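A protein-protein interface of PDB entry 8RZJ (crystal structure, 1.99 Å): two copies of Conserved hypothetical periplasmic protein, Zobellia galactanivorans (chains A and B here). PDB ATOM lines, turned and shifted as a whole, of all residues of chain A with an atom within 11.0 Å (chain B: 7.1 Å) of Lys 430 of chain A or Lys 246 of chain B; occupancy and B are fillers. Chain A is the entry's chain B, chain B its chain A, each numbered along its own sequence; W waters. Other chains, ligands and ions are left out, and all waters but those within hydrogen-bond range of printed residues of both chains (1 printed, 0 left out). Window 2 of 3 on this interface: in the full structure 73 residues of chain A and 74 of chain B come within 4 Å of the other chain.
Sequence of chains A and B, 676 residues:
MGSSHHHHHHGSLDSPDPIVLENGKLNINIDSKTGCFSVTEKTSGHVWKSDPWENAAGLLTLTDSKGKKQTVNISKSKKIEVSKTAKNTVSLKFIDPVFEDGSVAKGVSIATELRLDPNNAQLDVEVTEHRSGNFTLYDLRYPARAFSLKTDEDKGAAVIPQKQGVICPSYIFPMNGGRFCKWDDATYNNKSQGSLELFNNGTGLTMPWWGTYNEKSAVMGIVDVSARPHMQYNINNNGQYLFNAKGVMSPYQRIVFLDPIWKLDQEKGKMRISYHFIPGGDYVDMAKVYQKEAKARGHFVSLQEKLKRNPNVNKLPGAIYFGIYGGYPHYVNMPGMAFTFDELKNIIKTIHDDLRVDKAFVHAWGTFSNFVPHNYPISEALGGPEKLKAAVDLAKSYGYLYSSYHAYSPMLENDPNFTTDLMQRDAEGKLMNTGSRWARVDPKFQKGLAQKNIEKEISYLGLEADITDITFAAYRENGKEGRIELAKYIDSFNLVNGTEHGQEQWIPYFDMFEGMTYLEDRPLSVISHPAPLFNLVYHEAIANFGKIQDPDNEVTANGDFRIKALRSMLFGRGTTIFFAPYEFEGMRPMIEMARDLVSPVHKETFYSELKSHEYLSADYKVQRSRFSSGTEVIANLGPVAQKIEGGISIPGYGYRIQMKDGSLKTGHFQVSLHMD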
ATOM      1  N   THR A 420     -29.185   7.485 -12.190  1.00  0.00           N
ATOM      2  CA  THR A 420     -28.385   7.909 -11.053  1.00  0.00           C
ATOM      3  C   THR A 420     -29.237   8.206  -9.825  1.00  0.00           C
ATOM      4  O   THR A 420     -28.682   8.481  -8.757  1.00  0.00           O
ATOM      5  CB  THR A 420     -27.560   9.143 -11.430  1.00  0.00           C
ATOM      6  OG1 THR A 420     -28.439  10.184 -11.861  1.00  0.00           O
ATOM      7  CG2 THR A 420     -26.592   8.811 -12.557  1.00  0.00           C
ATOM      8  N   LEU A 422     -30.985   6.297  -7.941  1.00  0.00           N
ATOM      9  CA  LEU A 422     -30.761   5.333  -6.875  1.00  0.00           C
ATOM     10  C   LEU A 422     -29.323   5.330  -6.370  1.00  0.00           C
ATOM     11  O   LEU A 422     -28.987   4.497  -5.519  1.00  0.00           O
ATOM     12  CB  LEU A 422     -31.149   3.927  -7.350  1.00  0.00           C
ATOM     13  CG  LEU A 422     -32.651   3.679  -7.498  1.00  0.00           C
ATOM     14  CD1 LEU A 422     -32.918   2.503  -8.434  1.00  0.00           C
ATOM     15  CD2 LEU A 422     -33.285   3.433  -6.139  1.00  0.00           C
ATOM     16  N   MET A 423     -28.471   6.224  -6.867  1.00  0.00           N
ATOM     17  CA  MET A 423     -27.076   6.239  -6.447  1.00  0.00           C
ATOM     18  C   MET A 423     -26.869   7.228  -5.303  1.00  0.00           C
ATOM     19  O   MET A 423     -27.661   8.147  -5.086  1.00  0.00           O
ATOM     20  CB  MET A 423     -26.155   6.580  -7.628  1.00  0.00           C
ATOM     21  CG  MET A 423     -26.075   5.473  -8.689  1.00  0.00           C
ATOM     22  SD  MET A 423     -25.101   5.911 -10.154  1.00  0.00           S
ATOM     23  CE  MET A 423     -23.460   5.983  -9.428  1.00  0.00           C
ATOM     24  N   GLN A 424     -25.791   7.021  -4.562  1.00  0.00           N
ATOM     25  CA  GLN A 424     -25.449   7.875  -3.436  1.00  0.00           C
ATOM     26  C   GLN A 424     -24.485   8.968  -3.878  1.00  0.00           C
ATOM     27  O   GLN A 424     -23.681   8.773  -4.791  1.00  0.00           O
ATOM     28  CB  GLN A 424     -24.822   7.054  -2.311  1.00  0.00           C
ATOM     29  CG  GLN A 424     -24.568   7.847  -1.043  1.00  0.00           C
ATOM     30  CD  GLN A 424     -23.974   6.993   0.053  1.00  0.00           C
ATOM     31  OE1 GLN A 424     -23.695   5.809  -0.152  1.00  0.00           O
ATOM     32  NE2 GLN A 424     -23.774   7.589   1.227  1.00  0.00           N
ATOM     33  N   ARG A 425     -24.580  10.124  -3.225  1.00  0.00           N
ATOM     34  CA  ARG A 425     -23.696  11.255  -3.458  1.00  0.00           C
ATOM     35  C   ARG A 425     -22.969  11.629  -2.171  1.00  0.00           C
ATOM     36  O   ARG A 425     -23.505  11.477  -1.070  1.00  0.00           O
ATOM     37  CB  ARG A 425     -24.477  12.459  -3.984  1.00  0.00           C
ATOM     38  CG  ARG A 425     -25.032  12.240  -5.390  1.00  0.00           C
ATOM     39  CD  ARG A 425     -25.966  13.363  -5.841  1.00  0.00           C
ATOM     40  NE  ARG A 425     -26.559  13.062  -7.144  1.00  0.00           N
ATOM     41  CZ  ARG A 425     -25.980  13.352  -8.306  1.00  0.00           C
ATOM     42  NH1 ARG A 425     -24.795  13.953  -8.326  1.00  0.00           N
ATOM     43  NH2 ARG A 425     -26.579  13.039  -9.449  1.00  0.00           N
ATOM     44  N   ASP A 426     -21.741  12.134  -2.317  1.00  0.00           N
ATOM     45  CA  ASP A 426     -20.902  12.463  -1.173  1.00  0.00           C
ATOM     46  C   ASP A 426     -21.130  13.916  -0.754  1.00  0.00           C
ATOM     47  O   ASP A 426     -21.998  14.613  -1.289  1.00  0.00           O
ATOM     48  CB  ASP A 426     -19.432  12.171  -1.488  1.00  0.00           C
ATOM     49  CG  ASP A 426     -18.881  13.009  -2.650  1.00  0.00           C
ATOM     50  OD1 ASP A 426     -19.453  14.063  -3.012  1.00  0.00           O
ATOM     51  OD2 ASP A 426     -17.845  12.597  -3.206  1.00  0.00           O
ATOM     52  N   ALA A 427     -20.325  14.399   0.198  1.00  0.00           N
ATOM     53  CA  ALA A 427     -20.558  15.720   0.766  1.00  0.00           C
ATOM     54  C   ALA A 427     -20.430  16.827  -0.265  1.00  0.00           C
ATOM     55  O   ALA A 427     -20.955  17.927  -0.045  1.00  0.00           O
ATOM     56  CB  ALA A 427     -19.595  15.980   1.926  1.00  0.00           C
ATOM     57  N   GLU A 428     -19.749  16.570  -1.376  1.00  0.00           N
ATOM     58  CA  GLU A 428     -19.637  17.553  -2.444  1.00  0.00           C
ATOM     59  C   GLU A 428     -20.780  17.451  -3.435  1.00  0.00           C
ATOM     60  O   GLU A 428     -20.828  18.230  -4.390  1.00  0.00           O
ATOM     61  CB  GLU A 428     -18.309  17.394  -3.184  1.00  0.00           C
ATOM     62  CG  GLU A 428     -17.080  17.804  -2.389  1.00  0.00           C
ATOM     63  CD  GLU A 428     -15.842  17.936  -3.275  1.00  0.00           C
ATOM     64  OE1 GLU A 428     -15.234  16.891  -3.616  1.00  0.00           O
ATOM     65  OE2 GLU A 428     -15.492  19.085  -3.647  1.00  0.00           O
ATOM     66  N   GLY A 429     -21.693  16.507  -3.232  1.00  0.00           N
ATOM     67  CA  GLY A 429     -22.740  16.276  -4.199  1.00  0.00           C
ATOM     68  C   GLY A 429     -22.334  15.429  -5.383  1.00  0.00           C
ATOM     69  O   GLY A 429     -23.113  15.324  -6.335  1.00  0.00           O
ATOM     70  N   LYS A 430     -21.149  14.815  -5.356  1.00  0.00           N
ATOM     71  CA  LYS A 430     -20.682  13.990  -6.466  1.00  0.00           C
ATOM     72  C   LYS A 430     -21.114  12.541  -6.278  1.00  0.00           C
ATOM     73  O   LYS A 430     -21.136  12.034  -5.157  1.00  0.00           O
ATOM     74  CB  LYS A 430     -19.162  14.071  -6.594  1.00  0.00           C
ATOM     75  CG  LYS A 430     -18.653  15.499  -6.797  1.00  0.00           C
ATOM     76  CD  LYS A 430     -17.275  15.535  -7.442  1.00  0.00           C
ATOM     77  CE  LYS A 430     -16.170  15.664  -6.424  1.00  0.00           C
ATOM     78  NZ  LYS A 430     -16.184  14.516  -5.476  1.00  0.00           N
ATOM     79  N   LEU A 431     -21.459  11.881  -7.385  1.00  0.00           N
ATOM     80  CA  LEU A 431     -21.859  10.479  -7.329  1.00  0.00           C
ATOM     81  C   LEU A 431     -20.737   9.620  -6.775  1.00  0.00           C
ATOM     82  O   LEU A 431     -19.564   9.813  -7.102  1.00  0.00           O
ATOM     83  CB  LEU A 431     -22.236   9.968  -8.716  1.00  0.00           C
ATOM     84  CG  LEU A 431     -23.495  10.535  -9.366  1.00  0.00           C
ATOM     85  CD1 LEU A 431     -23.569  10.113 -10.831  1.00  0.00           C
ATOM     86  CD2 LEU A 431     -24.694  10.026  -8.581  1.00  0.00           C
ATOM     87  N   MET A 432     -21.110   8.656  -5.945  1.00  0.00           N
ATOM     88  CA  MET A 432     -20.179   7.684  -5.403  1.00  0.00           C
ATOM     89  C   MET A 432     -20.289   6.383  -6.184  1.00  0.00           C
ATOM     90  O   MET A 432     -21.338   6.061  -6.746  1.00  0.00           O
ATOM     91  CB  MET A 432     -20.455   7.430  -3.917  1.00  0.00           C
ATOM     92  CG  MET A 432     -20.372   8.698  -3.051  1.00  0.00           C
ATOM     93  SD  MET A 432     -20.997   8.441  -1.367  1.00  0.00           S
ATOM     94  CE  MET A 432     -20.190   6.899  -0.944  1.00  0.00           C
ATOM     95  N   ASN A 433     -19.176   5.651  -6.226  1.00  0.00           N
ATOM     96  CA  ASN A 433     -19.085   4.352  -6.889  1.00  0.00           C
ATOM     97  C   ASN A 433     -19.312   4.462  -8.393  1.00  0.00           C
ATOM     98  O   ASN A 433     -19.811   3.523  -9.021  1.00  0.00           O
ATOM     99  CB  ASN A 433     -20.057   3.342  -6.264  1.00  0.00           C
ATOM    100  CG  ASN A 433     -19.809   3.150  -4.774  1.00  0.00           C
ATOM    101  OD1 ASN A 433     -18.751   2.666  -4.373  1.00  0.00           O
ATOM    102  ND2 ASN A 433     -20.781   3.541  -3.946  1.00  0.00           N
ATOM    103  N   THR A 434     -18.950   5.604  -8.993  1.00  0.00           N
ATOM    104  CA  THR A 434     -18.992   5.668 -10.449  1.00  0.00           C
ATOM    105  C   THR A 434     -18.078   4.618 -11.063  1.00  0.00           C
ATOM    106  O   THR A 434     -18.354   4.119 -12.157  1.00  0.00           O
ATOM    107  CB  THR A 434     -18.629   7.074 -10.957  1.00  0.00           C
ATOM    108  OG1 THR A 434     -17.392   7.501 -10.382  1.00  0.00           O
ATOM    109  CG2 THR A 434     -19.707   8.061 -10.589  1.00  0.00           C
ATOM    110  N   GLY A 435     -17.018   4.230 -10.361  1.00  0.00           N
ATOM    111  CA  GLY A 435     -16.122   3.225 -10.891  1.00  0.00           C
ATOM    112  C   GLY A 435     -16.330   1.842 -10.312  1.00  0.00           C
ATOM    113  O   GLY A 435     -15.440   0.995 -10.413  1.00  0.00           O
ATOM    114  N   ARG A 440     -23.488   0.399  -6.730  1.00  0.00           N
ATOM    115  CA  ARG A 440     -23.876   1.783  -6.979  1.00  0.00           C
ATOM    116  C   ARG A 440     -25.164   2.194  -6.285  1.00  0.00           C
ATOM    117  O   ARG A 440     -25.340   3.381  -5.997  1.00  0.00           O
ATOM    118  CB  ARG A 440     -24.024   2.036  -8.486  1.00  0.00           C
ATOM    119  CG  ARG A 440     -22.697   2.266  -9.166  1.00  0.00           C
ATOM    120  CD  ARG A 440     -22.827   2.369 -10.658  1.00  0.00           C
ATOM    121  NE  ARG A 440     -21.524   2.538 -11.297  1.00  0.00           N
ATOM    122  CZ  ARG A 440     -21.302   2.285 -12.580  1.00  0.00           C
ATOM    123  NH1 ARG A 440     -22.299   1.843 -13.335  1.00  0.00           N
ATOM    124  NH2 ARG A 440     -20.090   2.448 -13.103  1.00  0.00           N
ATOM    125  N   ASP A 442     -27.565   3.003  -3.387  1.00  0.00           N
ATOM    126  CA  ASP A 442     -27.447   3.342  -1.972  1.00  0.00           C
ATOM    127  C   ASP A 442     -28.097   2.246  -1.128  1.00  0.00           C
ATOM    128  O   ASP A 442     -29.236   1.856  -1.406  1.00  0.00           O
ATOM    129  CB  ASP A 442     -28.119   4.691  -1.708  1.00  0.00           C
ATOM    130  CG  ASP A 442     -27.804   5.267  -0.325  1.00  0.00           C
ATOM    131  OD1 ASP A 442     -27.773   4.511   0.676  1.00  0.00           O
ATOM    132  OD2 ASP A 442     -27.606   6.503  -0.244  1.00  0.00           O
ATOM    133  N   ASN A 478     -20.256   3.698   6.072  1.00  0.00           N
ATOM    134  CA  ASN A 478     -21.209   4.398   5.227  1.00  0.00           C
ATOM    135  C   ASN A 478     -22.202   3.420   4.623  1.00  0.00           C
ATOM    136  O   ASN A 478     -21.811   2.494   3.906  1.00  0.00           O
ATOM    137  CB  ASN A 478     -20.496   5.152   4.118  1.00  0.00           C
ATOM    138  CG  ASN A 478     -21.469   5.749   3.139  1.00  0.00           C
ATOM    139  OD1 ASN A 478     -22.054   6.795   3.401  1.00  0.00           O
ATOM    140  ND2 ASN A 478     -21.679   5.069   2.019  1.00  0.00           N
ATOM    141  N   GLU B 100      -8.747  24.052 -19.178  1.00  0.00           N
ATOM    142  CA  GLU B 100     -10.134  23.837 -18.778  1.00  0.00           C
ATOM    143  C   GLU B 100     -10.779  25.129 -18.301  1.00  0.00           C
ATOM    144  O   GLU B 100     -11.949  25.394 -18.600  1.00  0.00           O
ATOM    145  CB  GLU B 100     -10.210  22.773 -17.683  1.00  0.00           C
ATOM    146  N   LEU B 242     -11.946   8.844 -16.688  1.00  0.00           N
ATOM    147  CA  LEU B 242     -11.792  10.277 -16.878  1.00  0.00           C
ATOM    148  C   LEU B 242     -12.751  11.070 -16.007  1.00  0.00           C
ATOM    149  O   LEU B 242     -12.559  12.277 -15.828  1.00  0.00           O
ATOM    150  CB  LEU B 242     -12.009  10.642 -18.350  1.00  0.00           C
ATOM    151  CG  LEU B 242     -11.026  10.004 -19.336  1.00  0.00           C
ATOM    152  CD1 LEU B 242     -11.436  10.268 -20.776  1.00  0.00           C
ATOM    153  CD2 LEU B 242      -9.600  10.485 -19.087  1.00  0.00           C
ATOM    154  N   PHE B 243     -13.769  10.421 -15.451  1.00  0.00           N
ATOM    155  CA  PHE B 243     -14.847  11.132 -14.789  1.00  0.00           C
ATOM    156  C   PHE B 243     -15.033  10.757 -13.331  1.00  0.00           C
ATOM    157  O   PHE B 243     -15.846  11.397 -12.654  1.00  0.00           O
ATOM    158  CB  PHE B 243     -16.175  10.897 -15.529  1.00  0.00           C
ATOM    159  CG  PHE B 243     -16.169  11.388 -16.952  1.00  0.00           C
ATOM    160  CD1 PHE B 243     -16.459  12.711 -17.244  1.00  0.00           C
ATOM    161  CD2 PHE B 243     -15.883  10.523 -17.995  1.00  0.00           C
ATOM    162  CE1 PHE B 243     -16.456  13.169 -18.558  1.00  0.00           C
ATOM    163  CE2 PHE B 243     -15.877  10.968 -19.308  1.00  0.00           C
ATOM    164  CZ  PHE B 243     -16.163  12.298 -19.589  1.00  0.00           C
ATOM    165  N   ASN B 244     -14.319   9.745 -12.829  1.00  0.00           N
ATOM    166  CA  ASN B 244     -14.530   9.316 -11.448  1.00  0.00           C
ATOM    167  C   ASN B 244     -14.251  10.447 -10.462  1.00  0.00           C
ATOM    168  O   ASN B 244     -14.976  10.610  -9.475  1.00  0.00           O
ATOM    169  CB  ASN B 244     -13.669   8.092 -11.137  1.00  0.00           C
ATOM    170  CG  ASN B 244     -14.210   6.820 -11.775  1.00  0.00           C
ATOM    171  OD1 ASN B 244     -15.410   6.701 -12.033  1.00  0.00           O
ATOM    172  ND2 ASN B 244     -13.327   5.861 -12.024  1.00  0.00           N
ATOM    173  N   ALA B 245     -13.214  11.251 -10.718  1.00  0.00           N
ATOM    174  CA  ALA B 245     -12.896  12.337  -9.793  1.00  0.00           C
ATOM    175  C   ALA B 245     -13.955  13.434  -9.830  1.00  0.00           C
ATOM    176  O   ALA B 245     -14.184  14.109  -8.821  1.00  0.00           O
ATOM    177  CB  ALA B 245     -11.512  12.912 -10.102  1.00  0.00           C
ATOM    178  N   LYS B 246     -14.615  13.620 -10.972  1.00  0.00           N
ATOM    179  CA  LYS B 246     -15.745  14.534 -11.034  1.00  0.00           C
ATOM    180  C   LYS B 246     -17.031  13.927 -10.487  1.00  0.00           C
ATOM    181  O   LYS B 246     -18.015  14.653 -10.331  1.00  0.00           O
ATOM    182  CB  LYS B 246     -15.975  14.994 -12.477  1.00  0.00           C
ATOM    183  CG  LYS B 246     -14.742  15.592 -13.144  1.00  0.00           C
ATOM    184  CD  LYS B 246     -15.010  15.964 -14.611  1.00  0.00           C
ATOM    185  CE  LYS B 246     -13.732  15.896 -15.456  1.00  0.00           C
ATOM    186  NZ  LYS B 246     -13.753  16.840 -16.620  1.00  0.00           N
ATOM    187  N   GLY B 247     -17.061  12.630 -10.200  1.00  0.00           N
ATOM    188  CA  GLY B 247     -18.298  12.028  -9.721  1.00  0.00           C
ATOM    189  C   GLY B 247     -19.464  12.120 -10.684  1.00  0.00           C
ATOM    190  O   GLY B 247     -20.592  12.405 -10.264  1.00  0.00           O
ATOM    191  N   VAL B 248     -19.218  11.889 -11.976  1.00  0.00           N
ATOM    192  CA  VAL B 248     -20.265  11.829 -12.985  1.00  0.00           C
ATOM    193  C   VAL B 248     -20.042  10.574 -13.819  1.00  0.00           C
ATOM    194  O   VAL B 248     -18.953  10.000 -13.835  1.00  0.00           O
ATOM    195  CB  VAL B 248     -20.290  13.081 -13.897  1.00  0.00           C
ATOM    196  CG1 VAL B 248     -20.183  14.364 -13.075  1.00  0.00           C
ATOM    197  CG2 VAL B 248     -19.169  13.014 -14.907  1.00  0.00           C
ATOM    198  N   MET B 249     -21.092  10.158 -14.523  1.00  0.00           N
ATOM    199  CA  MET B 249     -21.025   8.992 -15.405  1.00  0.00           C
ATOM    200  C   MET B 249     -20.428   9.372 -16.762  1.00  0.00           C
ATOM    201  O   MET B 249     -20.686  10.460 -17.281  1.00  0.00           O
ATOM    202  CB  MET B 249     -22.425   8.407 -15.602  1.00  0.00           C
ATOM    203  CG  MET B 249     -23.126   8.021 -14.306  1.00  0.00           C
ATOM    204  SD  MET B 249     -22.147   6.850 -13.330  1.00  0.00           S
ATOM    205  CE  MET B 249     -22.029   5.451 -14.450  1.00  0.00           C
HETATM  206  O   HOH W   1     -22.474  14.170 -10.127  1.00  0.00           O
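The side-chain amide oxygen (OD1) of Asn 244 of chain B lies within hydrogen-bond range of the side-chain hydroxyl (OG1) of Thr 434 of chain A, at 2.7 Å.
The backbone NH (N) of Gly 435 of chain A sits at hydrogen-bond distance from the side-chain amide oxygen (OD1) of Asn 244 of chain B (3.4 Å).
N of Leu 431 of chain A sits at hydrogen-bond distance from O of Gly 247 of chain B, at 3.1 Å.
The backbone carbonyl oxygen (O) of Phe 243 of chain B sits at hydrogen-bond distance from the backbone NH (N) of Val 248 of chain B, 3.5 Å away.
The side-chain carboxylate of Asp 426 of chain A is in salt-bridge range of the side-chain amino group of Lys 430 of chain A (3.4 Å).
OE1 of Glu 428 of chain A lies within salt-bridge range of NZ of Lys 430 of chain A, 3.2 Å away.
O of Asn 433 of chain A lies within hydrogen-bond range of NE of Arg 440 of chain A (3.0 Å).
O of Thr 434 of chain A is in hydrogen-bond range of NH2 of Arg 440 of chain A, at 2.6 Å.
Thr 420 of chain A touches Met 249 of chain B (CG2 to CG, 3.96 Å).
Lys 430 of chain A touches Ala 245 of chain B.
Lys 430 of chain A touches Lys 246 of chain B.
CA of Gly 247 of chain B touches CB of Lys 430 of chain A (3.8 Å).
Thr 434 of chain A touches Val 248 of chain B (CG2 to O, 3.9 Å).
Met 249 of chain B touches Thr 434 of chain A.
CZ of Arg 440 of chain A touches CE of Met 249 of chain B, 3.7 Å away.
Printed residues of chain A within 4 Å of Lys 246 of chain B: Lys 430.
No residue of chain A comes within 4 Å of Phe 243 of chain B.
Gly 247 of chain B touches just these residues of chain A: Lys 430 and Leu 431.
Val 248 of chain B touches just one residue of chain A: Thr 434.
Of the printed residues of chain B, Thr 434 of chain A touches Asn 244, Val 248 and Met 249.
Of the printed residues of chain B, Leu 431 of chain A touches Gly 247.
Asn 433 of chain A touches none of the printed residues of chain B.
Leu 422 of chain A touches none of the printed residues of chain B.
The nearest residue of chain B that does not touch Lys 430 of chain A is Asn 244 of chain B (5.7 Å).
The nearest residue of chain A that does not touch Lys 246 of chain B is Leu 431 of chain A (5.3 Å).
The nearest printed residue of chain B that does not touch Leu 431 of chain A is Met 249 of chain B (4.1 Å).
Hydrophobic or aromatic side chains of chain B within 4 Å of the printed part of chain A: Met 249.
Of the 18 printed residues of chain A, 6 touch a printed residue of chain B.
Hydrophobic or aromatic side chains of chain A that line the printed part of chain B: Leu 431.
Among the printed residues, 10 pairs touch across the chains.
Among the printed residues, no Asp or Glu carboxylate lies within 4 Å of a Lys or Arg side-chain nitrogen of the other chain.
No position is printed for both chains.
Water W1 bridges O of Gly 247 of chain B (2.6 Å) and NH1 of Arg 425 of chain A (2.9 Å).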
